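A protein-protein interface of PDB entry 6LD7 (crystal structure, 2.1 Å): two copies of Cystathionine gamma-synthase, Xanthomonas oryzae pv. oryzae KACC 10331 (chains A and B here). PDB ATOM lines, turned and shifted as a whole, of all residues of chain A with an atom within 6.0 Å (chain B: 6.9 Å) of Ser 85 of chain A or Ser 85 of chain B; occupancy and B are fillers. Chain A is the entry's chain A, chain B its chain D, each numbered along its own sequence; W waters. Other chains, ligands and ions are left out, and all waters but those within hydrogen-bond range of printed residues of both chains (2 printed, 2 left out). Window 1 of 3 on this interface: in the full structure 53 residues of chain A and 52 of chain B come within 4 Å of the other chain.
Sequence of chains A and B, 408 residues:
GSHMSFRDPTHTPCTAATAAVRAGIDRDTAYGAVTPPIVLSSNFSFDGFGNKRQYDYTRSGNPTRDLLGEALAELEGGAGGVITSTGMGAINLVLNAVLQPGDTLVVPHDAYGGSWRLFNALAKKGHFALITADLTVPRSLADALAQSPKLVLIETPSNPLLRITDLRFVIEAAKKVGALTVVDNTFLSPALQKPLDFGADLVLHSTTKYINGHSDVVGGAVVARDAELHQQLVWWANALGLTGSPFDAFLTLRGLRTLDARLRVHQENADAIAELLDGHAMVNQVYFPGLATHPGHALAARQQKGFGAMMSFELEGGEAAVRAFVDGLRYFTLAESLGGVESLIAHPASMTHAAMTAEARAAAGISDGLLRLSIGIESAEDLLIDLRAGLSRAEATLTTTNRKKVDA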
ATOM      1  N   ILE A  83       7.155  23.578 -12.223  1.00  0.00           N
ATOM      2  CA  ILE A  83       5.854  22.953 -12.555  1.00  0.00           C
ATOM      3  C   ILE A  83       4.735  23.711 -11.875  1.00  0.00           C
ATOM      4  O   ILE A  83       4.717  23.773 -10.629  1.00  0.00           O
ATOM      5  CB  ILE A  83       5.901  21.439 -12.178  1.00  0.00           C
ATOM      6  CG1 ILE A  83       7.080  20.701 -12.816  1.00  0.00           C
ATOM      7  CG2 ILE A  83       4.592  20.777 -12.589  1.00  0.00           C
ATOM      8  CD1 ILE A  83       7.163  20.829 -14.386  1.00  0.00           C
ATOM      9  N   THR A  84       3.758  24.120 -12.643  1.00  0.00           N
ATOM     10  CA  THR A  84       2.646  24.996 -12.231  1.00  0.00           C
ATOM     11  C   THR A  84       1.365  24.177 -12.311  1.00  0.00           C
ATOM     12  O   THR A  84       1.342  23.124 -13.027  1.00  0.00           O
ATOM     13  CB  THR A  84       2.594  26.248 -13.154  1.00  0.00           C
ATOM     14  OG1 THR A  84       2.480  25.884 -14.531  1.00  0.00           O
ATOM     15  CG2 THR A  84       3.872  27.059 -12.991  1.00  0.00           C
ATOM     16  N   SER A  85       0.313  24.696 -11.734  1.00  0.00           N
ATOM     17  CA  SER A  85      -1.011  24.010 -11.736  1.00  0.00           C
ATOM     18  C   SER A  85      -1.668  23.988 -13.117  1.00  0.00           C
ATOM     19  O   SER A  85      -2.462  23.071 -13.369  1.00  0.00           O
ATOM     20  CB  SER A  85      -1.917  24.611 -10.704  1.00  0.00           C
ATOM     21  OG  SER A  85      -1.902  26.028 -10.850  1.00  0.00           O
ATOM     22  N   THR A  86      -1.346  24.937 -13.993  1.00  0.00           N
ATOM     23  CA  THR A  86      -1.915  25.008 -15.352  1.00  0.00           C
ATOM     24  C   THR A  86      -0.870  25.615 -16.278  1.00  0.00           C
ATOM     25  O   THR A  86       0.160  26.288 -15.778  1.00  0.00           O
ATOM     26  CB  THR A  86      -3.232  25.833 -15.390  1.00  0.00           C
ATOM     27  OG1 THR A  86      -2.965  27.215 -15.135  1.00  0.00           O
ATOM     28  CG2 THR A  86      -4.292  25.404 -14.375  1.00  0.00           C
ATOM     29  N   GLY A  87      -1.149  25.540 -17.588  1.00  0.00           N
ATOM     30  CA  GLY A  87      -0.267  26.212 -18.559  1.00  0.00           C
ATOM     31  C   GLY A  87      -0.433  27.714 -18.422  1.00  0.00           C
ATOM     32  O   GLY A  87       0.620  28.425 -18.464  1.00  0.00           O
ATOM     33  N   GLY A  89      -0.975  29.295 -15.829  1.00  0.00           N
ATOM     34  CA  GLY A  89      -0.183  29.567 -14.633  1.00  0.00           C
ATOM     35  C   GLY A  89       1.275  29.743 -14.948  1.00  0.00           C
ATOM     36  O   GLY A  89       1.968  30.482 -14.232  1.00  0.00           O
ATOM     37  N   VAL A 218      -4.375  18.726 -15.939  1.00  0.00           N
ATOM     38  CA  VAL A 218      -4.114  20.086 -16.414  1.00  0.00           C
ATOM     39  C   VAL A 218      -2.873  20.550 -15.674  1.00  0.00           C
ATOM     40  O   VAL A 218      -2.852  20.353 -14.479  1.00  0.00           O
ATOM     41  CB  VAL A 218      -5.313  21.000 -16.142  1.00  0.00           C
ATOM     42  CG1 VAL A 218      -4.955  22.438 -16.562  1.00  0.00           C
ATOM     43  CG2 VAL A 218      -6.537  20.506 -16.884  1.00  0.00           C
ATOM     44  N   GLY A 219      -1.864  21.090 -16.377  1.00  0.00           N
ATOM     45  CA  GLY A 219      -0.596  21.500 -15.754  1.00  0.00           C
ATOM     46  C   GLY A 219       0.245  22.405 -16.665  1.00  0.00           C
ATOM     47  O   GLY A 219      -0.051  22.508 -17.862  1.00  0.00           O
ATOM     48  N   GLY A 220       1.299  22.997 -16.128  1.00  0.00           N
ATOM     49  CA  GLY A 220       2.237  23.762 -16.961  1.00  0.00           C
ATOM     50  C   GLY A 220       3.643  23.560 -16.505  1.00  0.00           C
ATOM     51  O   GLY A 220       3.876  23.016 -15.377  1.00  0.00           O
ATOM     52  N   GLY A 241       2.038  31.140  -5.155  1.00  0.00           N
ATOM     53  CA  GLY A 241       1.204  29.923  -4.962  1.00  0.00           C
ATOM     54  C   GLY A 241       0.728  29.258  -6.247  1.00  0.00           C
ATOM     55  O   GLY A 241      -0.374  28.662  -6.239  1.00  0.00           O
ATOM     56  N   LEU A 242       1.565  29.289  -7.284  1.00  0.00           N
ATOM     57  CA  LEU A 242       1.294  28.751  -8.635  1.00  0.00           C
ATOM     58  C   LEU A 242       1.762  27.304  -8.815  1.00  0.00           C
ATOM     59  O   LEU A 242       1.461  26.771  -9.907  1.00  0.00           O
ATOM     60  CB  LEU A 242       2.022  29.633  -9.684  1.00  0.00           C
ATOM     61  CG  LEU A 242       1.357  30.969  -9.939  1.00  0.00           C
ATOM     62  CD1 LEU A 242       2.187  31.826 -10.874  1.00  0.00           C
ATOM     63  CD2 LEU A 242      -0.028  30.760 -10.515  1.00  0.00           C
ATOM     64  N   THR A 243       2.453  26.687  -7.866  1.00  0.00           N
ATOM     65  CA  THR A 243       2.966  25.294  -7.984  1.00  0.00           C
ATOM     66  C   THR A 243       1.833  24.243  -8.084  1.00  0.00           C
ATOM     67  O   THR A 243       0.770  24.497  -7.616  1.00  0.00           O
ATOM     68  CB  THR A 243       3.950  24.968  -6.865  1.00  0.00           C
ATOM     69  OG1 THR A 243       3.374  25.280  -5.589  1.00  0.00           O
ATOM     70  CG2 THR A 243       5.242  25.749  -7.023  1.00  0.00           C
ATOM     71  N   GLY A 244       2.106  23.164  -8.822  1.00  0.00           N
ATOM     72  CA  GLY A 244       1.183  22.059  -9.115  1.00  0.00           C
ATOM     73  C   GLY A 244       1.163  20.939  -8.043  1.00  0.00           C
ATOM     74  O   GLY A 244       2.102  20.755  -7.259  1.00  0.00           O
ATOM     75  N   SER A 245       0.116  20.172  -8.098  1.00  0.00           N
ATOM     76  CA  SER A 245      -0.114  18.973  -7.286  1.00  0.00           C
ATOM     77  C   SER A 245       0.963  17.925  -7.628  1.00  0.00           C
ATOM     78  O   SER A 245       1.204  17.623  -8.807  1.00  0.00           O
ATOM     79  CB  SER A 245      -1.491  18.457  -7.633  1.00  0.00           C
ATOM     80  OG  SER A 245      -1.587  17.064  -7.320  1.00  0.00           O
ATOM     81  N   ASP A 248      -0.584  15.069  -9.881  1.00  0.00           N
ATOM     82  CA  ASP A 248      -0.529  15.552 -11.292  1.00  0.00           C
ATOM     83  C   ASP A 248       0.862  15.409 -11.883  1.00  0.00           C
ATOM     84  O   ASP A 248       0.971  14.975 -13.042  1.00  0.00           O
ATOM     85  CB  ASP A 248      -1.068  16.967 -11.404  1.00  0.00           C
ATOM     86  CG  ASP A 248      -2.574  17.027 -11.293  1.00  0.00           C
ATOM     87  OD1 ASP A 248      -3.131  15.979 -10.851  1.00  0.00           O
ATOM     88  OD2 ASP A 248      -3.185  18.131 -11.657  1.00  0.00           O
ATOM     89  N   ARG B  59      -9.435  23.579 -16.618  1.00  0.00           N
ATOM     90  CA  ARG B  59      -8.841  24.802 -16.006  1.00  0.00           C
ATOM     91  C   ARG B  59      -9.991  25.760 -15.590  1.00  0.00           C
ATOM     92  O   ARG B  59      -9.834  26.499 -14.584  1.00  0.00           O
ATOM     93  CB  ARG B  59      -7.786  25.490 -16.910  1.00  0.00           C
ATOM     94  CG  ARG B  59      -7.536  26.946 -16.492  1.00  0.00           C
ATOM     95  CD  ARG B  59      -6.368  27.682 -17.067  1.00  0.00           C
ATOM     96  NE  ARG B  59      -6.155  27.317 -18.471  1.00  0.00           N
ATOM     97  CZ  ARG B  59      -6.866  27.725 -19.527  1.00  0.00           C
ATOM     98  NH1 ARG B  59      -7.872  28.563 -19.391  1.00  0.00           N
ATOM     99  NH2 ARG B  59      -6.503  27.354 -20.746  1.00  0.00           N
ATOM    100  N   ILE B  83     -11.680  26.974  -5.853  1.00  0.00           N
ATOM    101  CA  ILE B  83     -10.606  26.100  -5.313  1.00  0.00           C
ATOM    102  C   ILE B  83      -9.326  26.339  -6.090  1.00  0.00           C
ATOM    103  O   ILE B  83      -9.298  26.121  -7.325  1.00  0.00           O
ATOM    104  CB  ILE B  83     -11.061  24.623  -5.365  1.00  0.00           C
ATOM    105  CG1 ILE B  83     -12.385  24.372  -4.644  1.00  0.00           C
ATOM    106  CG2 ILE B  83      -9.976  23.746  -4.736  1.00  0.00           C
ATOM    107  CD1 ILE B  83     -12.415  24.822  -3.154  1.00  0.00           C
ATOM    108  N   THR B  84      -8.271  26.662  -5.394  1.00  0.00           N
ATOM    109  CA  THR B  84      -6.983  27.084  -5.988  1.00  0.00           C
ATOM    110  C   THR B  84      -5.938  26.023  -5.674  1.00  0.00           C
ATOM    111  O   THR B  84      -6.142  25.203  -4.742  1.00  0.00           O
ATOM    112  CB  THR B  84      -6.551  28.440  -5.386  1.00  0.00           C
ATOM    113  OG1 THR B  84      -6.491  28.398  -3.958  1.00  0.00           O
ATOM    114  CG2 THR B  84      -7.515  29.535  -5.804  1.00  0.00           C
ATOM    115  N   SER B  85      -4.819  26.071  -6.344  1.00  0.00           N
ATOM    116  CA  SER B  85      -3.748  25.056  -6.161  1.00  0.00           C
ATOM    117  C   SER B  85      -3.071  25.170  -4.788  1.00  0.00           C
ATOM    118  O   SER B  85      -2.571  24.153  -4.316  1.00  0.00           O
ATOM    119  CB  SER B  85      -2.749  25.098  -7.292  1.00  0.00           C
ATOM    120  OG  SER B  85      -2.209  26.403  -7.361  1.00  0.00           O
ATOM    121  N   THR B  86      -3.089  26.352  -4.157  1.00  0.00           N
ATOM    122  CA  THR B  86      -2.479  26.574  -2.819  1.00  0.00           C
ATOM    123  C   THR B  86      -3.277  27.663  -2.094  1.00  0.00           C
ATOM    124  O   THR B  86      -4.111  28.473  -2.761  1.00  0.00           O
ATOM    125  CB  THR B  86      -0.975  26.940  -2.918  1.00  0.00           C
ATOM    126  OG1 THR B  86      -0.865  28.272  -3.434  1.00  0.00           O
ATOM    127  CG2 THR B  86      -0.171  26.020  -3.833  1.00  0.00           C
ATOM    128  N   GLY B  87      -3.015  27.768  -0.785  1.00  0.00           N
ATOM    129  CA  GLY B  87      -3.606  28.870  -0.003  1.00  0.00           C
ATOM    130  C   GLY B  87      -3.041  30.184  -0.486  1.00  0.00           C
ATOM    131  O   GLY B  87      -3.837  31.144  -0.634  1.00  0.00           O
ATOM    132  N   MET B  88      -1.738  30.246  -0.695  1.00  0.00           N
ATOM    133  CA  MET B  88      -1.148  31.506  -1.277  1.00  0.00           C
ATOM    134  C   MET B  88      -1.850  31.904  -2.582  1.00  0.00           C
ATOM    135  O   MET B  88      -2.055  33.081  -2.828  1.00  0.00           O
ATOM    136  CB  MET B  88       0.356  31.392  -1.478  1.00  0.00           C
ATOM    137  CG  MET B  88       1.158  31.536  -0.172  1.00  0.00           C
ATOM    138  SD  MET B  88       0.636  32.916   0.953  1.00  0.00           S
ATOM    139  CE  MET B  88       0.521  34.161  -0.335  1.00  0.00           C
ATOM    140  N   GLY B  89      -2.221  30.918  -3.389  1.00  0.00           N
ATOM    141  CA  GLY B  89      -2.933  31.153  -4.631  1.00  0.00           C
ATOM    142  C   GLY B  89      -4.261  31.793  -4.381  1.00  0.00           C
ATOM    143  O   GLY B  89      -4.747  32.531  -5.229  1.00  0.00           O
ATOM    144  N   ALA B  90      -4.944  31.376  -3.348  1.00  0.00           N
ATOM    145  CA  ALA B  90      -6.260  31.941  -3.015  1.00  0.00           C
ATOM    146  C   ALA B  90      -6.083  33.414  -2.667  1.00  0.00           C
ATOM    147  O   ALA B  90      -6.967  34.196  -3.014  1.00  0.00           O
ATOM    148  CB  ALA B  90      -6.854  31.207  -1.850  1.00  0.00           C
ATOM    149  N   THR B 207      -6.543  25.081   2.451  1.00  0.00           N
ATOM    150  CA  THR B 207      -7.190  23.767   2.729  1.00  0.00           C
ATOM    151  C   THR B 207      -6.115  22.770   3.115  1.00  0.00           C
ATOM    152  O   THR B 207      -6.437  21.717   3.693  1.00  0.00           O
ATOM    153  CB  THR B 207      -8.004  23.276   1.541  1.00  0.00           C
ATOM    154  OG1 THR B 207      -7.082  23.153   0.480  1.00  0.00           O
ATOM    155  CG2 THR B 207      -9.081  24.257   1.199  1.00  0.00           C
ATOM    156  N   THR B 208      -4.857  23.182   3.009  1.00  0.00           N
ATOM    157  CA  THR B 208      -3.664  22.372   3.390  1.00  0.00           C
ATOM    158  C   THR B 208      -3.742  21.932   4.865  1.00  0.00           C
ATOM    159  O   THR B 208      -2.982  21.050   5.294  1.00  0.00           O
ATOM    160  CB  THR B 208      -2.429  23.216   3.077  1.00  0.00           C
ATOM    161  OG1 THR B 208      -2.525  23.706   1.710  1.00  0.00           O
ATOM    162  CG2 THR B 208      -1.156  22.435   3.318  1.00  0.00           C
ATOM    163  N1  LLP B 209      -2.862  31.689   5.416  1.00  0.00           N
ATOM    164  C2  LLP B 209      -2.582  31.136   6.594  1.00  0.00           C
ATOM    165  C2' LLP B 209      -3.165  31.724   7.862  1.00  0.00           C
ATOM    166  C3  LLP B 209      -1.767  29.993   6.632  1.00  0.00           C
ATOM    167  O3  LLP B 209      -1.578  29.400   7.809  1.00  0.00           O
ATOM    168  C4  LLP B 209      -1.204  29.435   5.461  1.00  0.00           C
ATOM    169  C4' LLP B 209      -0.434  28.148   5.620  1.00  0.00           C
ATOM    170  C5  LLP B 209      -1.481  30.085   4.255  1.00  0.00           C
ATOM    171  C6  LLP B 209      -2.282  31.202   4.290  1.00  0.00           C
ATOM    172  C5' LLP B 209      -0.863  29.658   2.942  1.00  0.00           C
ATOM    173  OP4 LLP B 209      -1.448  28.465   2.370  1.00  0.00           O
ATOM    174  P   LLP B 209      -0.621  27.383   1.509  1.00  0.00           P
ATOM    175  OP1 LLP B 209      -1.675  26.250   1.323  1.00  0.00           O
ATOM    176  OP2 LLP B 209       0.581  27.010   2.337  1.00  0.00           O
ATOM    177  OP3 LLP B 209      -0.293  28.162   0.130  1.00  0.00           O
ATOM    178  N   LLP B 209      -4.419  22.770   5.664  1.00  0.00           N
ATOM    179  CA  LLP B 209      -4.347  22.718   7.130  1.00  0.00           C
ATOM    180  CB  LLP B 209      -4.181  24.145   7.697  1.00  0.00           C
ATOM    181  CG  LLP B 209      -2.761  24.734   7.663  1.00  0.00           C
ATOM    182  CD  LLP B 209      -2.079  25.061   6.372  1.00  0.00           C
ATOM    183  CE  LLP B 209      -0.652  25.748   6.507  1.00  0.00           C
ATOM    184  NZ  LLP B 209      -0.803  27.222   6.593  1.00  0.00           N
ATOM    185  C   LLP B 209      -5.525  21.856   7.604  1.00  0.00           C
ATOM    186  O   LLP B 209      -5.514  20.691   7.229  1.00  0.00           O
ATOM    187  N   VAL B 217      -2.264  17.191   1.007  1.00  0.00           N
ATOM    188  CA  VAL B 217      -2.727  18.087  -0.073  1.00  0.00           C
ATOM    189  C   VAL B 217      -2.308  19.472   0.276  1.00  0.00           C
ATOM    190  O   VAL B 217      -2.477  19.889   1.486  1.00  0.00           O
ATOM    191  CB  VAL B 217      -4.241  18.096  -0.171  1.00  0.00           C
ATOM    192  CG1 VAL B 217      -4.679  19.253  -1.047  1.00  0.00           C
ATOM    193  CG2 VAL B 217      -4.736  16.749  -0.642  1.00  0.00           C
ATOM    194  N   VAL B 218      -1.791  20.159  -0.709  1.00  0.00           N
ATOM    195  CA  VAL B 218      -1.658  21.611  -0.591  1.00  0.00           C
ATOM    196  C   VAL B 218      -2.752  22.230  -1.454  1.00  0.00           C
ATOM    197  O   VAL B 218      -2.933  21.757  -2.583  1.00  0.00           O
ATOM    198  CB  VAL B 218      -0.268  22.063  -1.039  1.00  0.00           C
ATOM    199  CG1 VAL B 218      -0.172  23.607  -0.983  1.00  0.00           C
ATOM    200  CG2 VAL B 218       0.811  21.416  -0.193  1.00  0.00           C
ATOM    201  N   GLY B 219      -3.522  23.172  -0.920  1.00  0.00           N
ATOM    202  CA  GLY B 219      -4.688  23.737  -1.658  1.00  0.00           C
ATOM    203  C   GLY B 219      -5.220  25.023  -1.008  1.00  0.00           C
ATOM    204  O   GLY B 219      -4.842  25.290   0.125  1.00  0.00           O
ATOM    205  N   GLY B 220      -6.117  25.753  -1.673  1.00  0.00           N
ATOM    206  CA  GLY B 220      -6.749  26.943  -1.092  1.00  0.00           C
ATOM    207  C   GLY B 220      -8.165  27.035  -1.568  1.00  0.00           C
ATOM    208  O   GLY B 220      -8.558  26.285  -2.505  1.00  0.00           O
ATOM    209  N   LEU B 240      -5.913  33.548 -14.754  1.00  0.00           N
ATOM    210  CA  LEU B 240      -4.576  33.464 -14.141  1.00  0.00           C
ATOM    211  C   LEU B 240      -4.097  31.999 -14.058  1.00  0.00           C
ATOM    212  O   LEU B 240      -2.908  31.779 -13.741  1.00  0.00           O
ATOM    213  CB  LEU B 240      -4.648  34.057 -12.743  1.00  0.00           C
ATOM    214  CG  LEU B 240      -4.972  35.540 -12.643  1.00  0.00           C
ATOM    215  CD1 LEU B 240      -5.396  35.951 -11.248  1.00  0.00           C
ATOM    216  CD2 LEU B 240      -3.786  36.374 -12.991  1.00  0.00           C
ATOM    217  N   GLY B 241      -4.943  31.014 -14.319  1.00  0.00           N
ATOM    218  CA  GLY B 241      -4.454  29.623 -14.190  1.00  0.00           C
ATOM    219  C   GLY B 241      -4.165  29.170 -12.747  1.00  0.00           C
ATOM    220  O   GLY B 241      -3.259  28.293 -12.555  1.00  0.00           O
ATOM    221  N   LEU B 242      -4.918  29.696 -11.769  1.00  0.00           N
ATOM    222  CA  LEU B 242      -4.738  29.405 -10.331  1.00  0.00           C
ATOM    223  C   LEU B 242      -5.573  28.204  -9.848  1.00  0.00           C
ATOM    224  O   LEU B 242      -5.416  27.896  -8.656  1.00  0.00           O
ATOM    225  CB  LEU B 242      -5.156  30.658  -9.525  1.00  0.00           C
ATOM    226  CG  LEU B 242      -4.129  31.767  -9.574  1.00  0.00           C
ATOM    227  CD1 LEU B 242      -4.662  33.034  -8.914  1.00  0.00           C
ATOM    228  CD2 LEU B 242      -2.857  31.306  -8.898  1.00  0.00           C
ATOM    229  N   THR B 243      -6.454  27.613 -10.638  1.00  0.00           N
ATOM    230  CA  THR B 243      -7.332  26.475 -10.220  1.00  0.00           C
ATOM    231  C   THR B 243      -6.557  25.202  -9.834  1.00  0.00           C
ATOM    232  O   THR B 243      -5.516  25.004 -10.357  1.00  0.00           O
ATOM    233  CB  THR B 243      -8.396  26.149 -11.261  1.00  0.00           C
ATOM    234  OG1 THR B 243      -7.791  25.994 -12.551  1.00  0.00           O
ATOM    235  CG2 THR B 243      -9.432  27.261 -11.374  1.00  0.00           C
ATOM    236  N   GLY B 244      -7.091  24.438  -8.860  1.00  0.00           N
ATOM    237  CA  GLY B 244      -6.446  23.226  -8.332  1.00  0.00           C
ATOM    238  C   GLY B 244      -6.745  21.947  -9.151  1.00  0.00           C
ATOM    239  O   GLY B 244      -7.729  21.852  -9.845  1.00  0.00           O
ATOM    240  N   SER B 245      -5.947  20.948  -8.924  1.00  0.00           N
ATOM    241  CA  SER B 245      -6.108  19.561  -9.387  1.00  0.00           C
ATOM    242  C   SER B 245      -7.404  18.942  -8.820  1.00  0.00           C
ATOM    243  O   SER B 245      -7.692  19.003  -7.620  1.00  0.00           O
ATOM    244  CB  SER B 245      -4.897  18.804  -8.908  1.00  0.00           C
ATOM    245  OG  SER B 245      -5.193  17.415  -8.892  1.00  0.00           O
ATOM    246  N   ASP B 248      -6.615  16.393  -5.964  1.00  0.00           N
ATOM    247  CA  ASP B 248      -6.484  17.171  -4.692  1.00  0.00           C
ATOM    248  C   ASP B 248      -7.833  17.524  -4.090  1.00  0.00           C
ATOM    249  O   ASP B 248      -8.048  17.403  -2.823  1.00  0.00           O
ATOM    250  CB  ASP B 248      -5.572  18.390  -4.888  1.00  0.00           C
ATOM    251  CG  ASP B 248      -4.080  18.020  -4.912  1.00  0.00           C
ATOM    252  OD1 ASP B 248      -3.803  16.774  -4.983  1.00  0.00           O
ATOM    253  OD2 ASP B 248      -3.192  18.942  -4.803  1.00  0.00           O
HETATM  254  O   HOH W   1      -5.851  15.861 -10.734  1.00  0.00           O
HETATM  255  O   HOH W   2      -1.329  15.917  -5.022  1.00  0.00           O
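OG of Ser 245 of chain A is in hydrogen-bond range of N of Asp 248 of chain A (3.4 Å).
The side-chain hydroxyl of Thr 84 of chain B lies within hydrogen-bond range of the backbone carbonyl oxygen of Thr 86 of chain B, 2.7 Å away.
The backbone NH (N) of Ser 85 of chain B sits at hydrogen-bond distance from the backbone carbonyl oxygen (O) of Leu 242 of chain B.
OG1 of Thr 86 of chain B lies within hydrogen-bond range of N of Gly 89 of chain B, at 3.0 Å.
OP3 of LLP 209 of chain B lies within hydrogen-bond range of the backbone NH (N) of Met 88 of chain B.
The side-chain hydroxyl (OG) of Ser 245 of chain B lies within hydrogen-bond range of the backbone NH (N) of Asp 248 of chain B.
Ser 85 of chain A touches its own counterpart, Ser 85 of chain B.
Ser 85 of chain A touches Gly 241 of chain B, and with the chains exchanged Gly 241 of chain A touches Ser 85 of chain B.
Thr 86 of chain A touches Gly 241 of chain B, and with the chains exchanged Gly 241 of chain A touches Thr 86 of chain B.
Leu 242 of chain A touches its own counterpart, Leu 242 of chain B.
Water W1 bridges the side-chain hydroxyl (OG) of Ser 245 of chain B and the side-chain carboxylate (OD1) of Asp 248 of chain A.
Water W2 bridges OG of Ser 245 of chain A and OD1 of Asp 248 of chain B.
Ser 85 of chain A touches three residues of chain B.
Ser 85 of chain B touches just these residues of chain A: Ser 85 (3.5 Å), Gly 241 (3.1 Å) and Thr 243 (3.5 Å).
Printed residues of chain B within 4 Å of Gly 241 of chain A: Ser 85 (3.1 Å), Thr 86 (2.9 Å), Met 88 (3.9 Å) and Gly 89 (3.9 Å).
Printed residues of chain A within 4 Å of Leu 240 of chain B: Gly 89 (3.6 Å).
Printed residues of chain A within 4 Å of Asp 248 of chain B: Ser 245 (3.2 Å).
Of the printed residues of chain A, Leu 242 of chain B touches Leu 242 (3.3 Å).
Printed residues of chain B within 4 Å of Thr 243 of chain A: Ser 85 (3.5 Å).
Gly 87 of chain B touches none of the printed residues of chain A.
The nearest residue of chain A that does not touch Ser 85 of chain B is Leu 242 of chain A (4.3 Å).
The nearest printed residue of chain B that does not touch Gly 89 of chain A is Leu 242 of chain B (5.5 Å).
OG of Ser 85 of chain B touches OG of Ser 85 of chain A, at 3.5 Å.
CB of Ser 85 of chain A touches O of Thr 243 of chain B (3.6 Å).
Thr 86 of chain A touches Arg 59 of chain B (OG1 to CD, 3.9 Å).
Thr 243 of chain B touches Thr 86 of chain A (OG1 to CG2, 3.99 Å).
Leu 240 of chain B touches Gly 89 of chain A (O to CA, 3.6 Å).
Gly 241 of chain B touches Gly 89 of chain A (CA to N, 3.9 Å).
Gly 241 of chain A touches Met 88 of chain B.
N of Gly 89 of chain B touches CA of Gly 241 of chain A, 3.9 Å away.
Ser 85 of chain B touches Thr 243 of chain A.
CB of Ser 245 of chain B touches CB of Ser 245 of chain A (3.7 Å).
Of the 15 printed residues of chain A, 8 touch a printed residue of chain B.
Of the 23 printed residues of chain B, 11 touch a printed residue of chain A.
Among the printed residues, no Asp or Glu carboxylate lies within 4 Å of a Lys or Arg side-chain nitrogen of the other chain.
The side-chain hydroxyl (OG) of Ser 85 of chain A lies within hydrogen-bond range of the backbone carbonyl oxygen (O) of Gly 241 of chain B (3.1 Å).
O of Gly 241 of chain B is in hydrogen-bond range of OG1 of Thr 86 of chain A.
The backbone carbonyl oxygen of Gly 241 of chain A sits at hydrogen-bond distance from the side-chain hydroxyl of Ser 85 of chain B.
O of Gly 241 of chain A is in hydrogen-bond range of OG1 of Thr 86 of chain B (2.9 Å).
The side-chain hydroxyl (OG) of Ser 245 of chain A sits at hydrogen-bond distance from the side-chain carboxylate (OD1) of Asp 248 of chain B, 3.2 Å away.
OD1 of Asp 248 of chain A is in hydrogen-bond range of OG of Ser 245 of chain B, 3.2 Å away.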
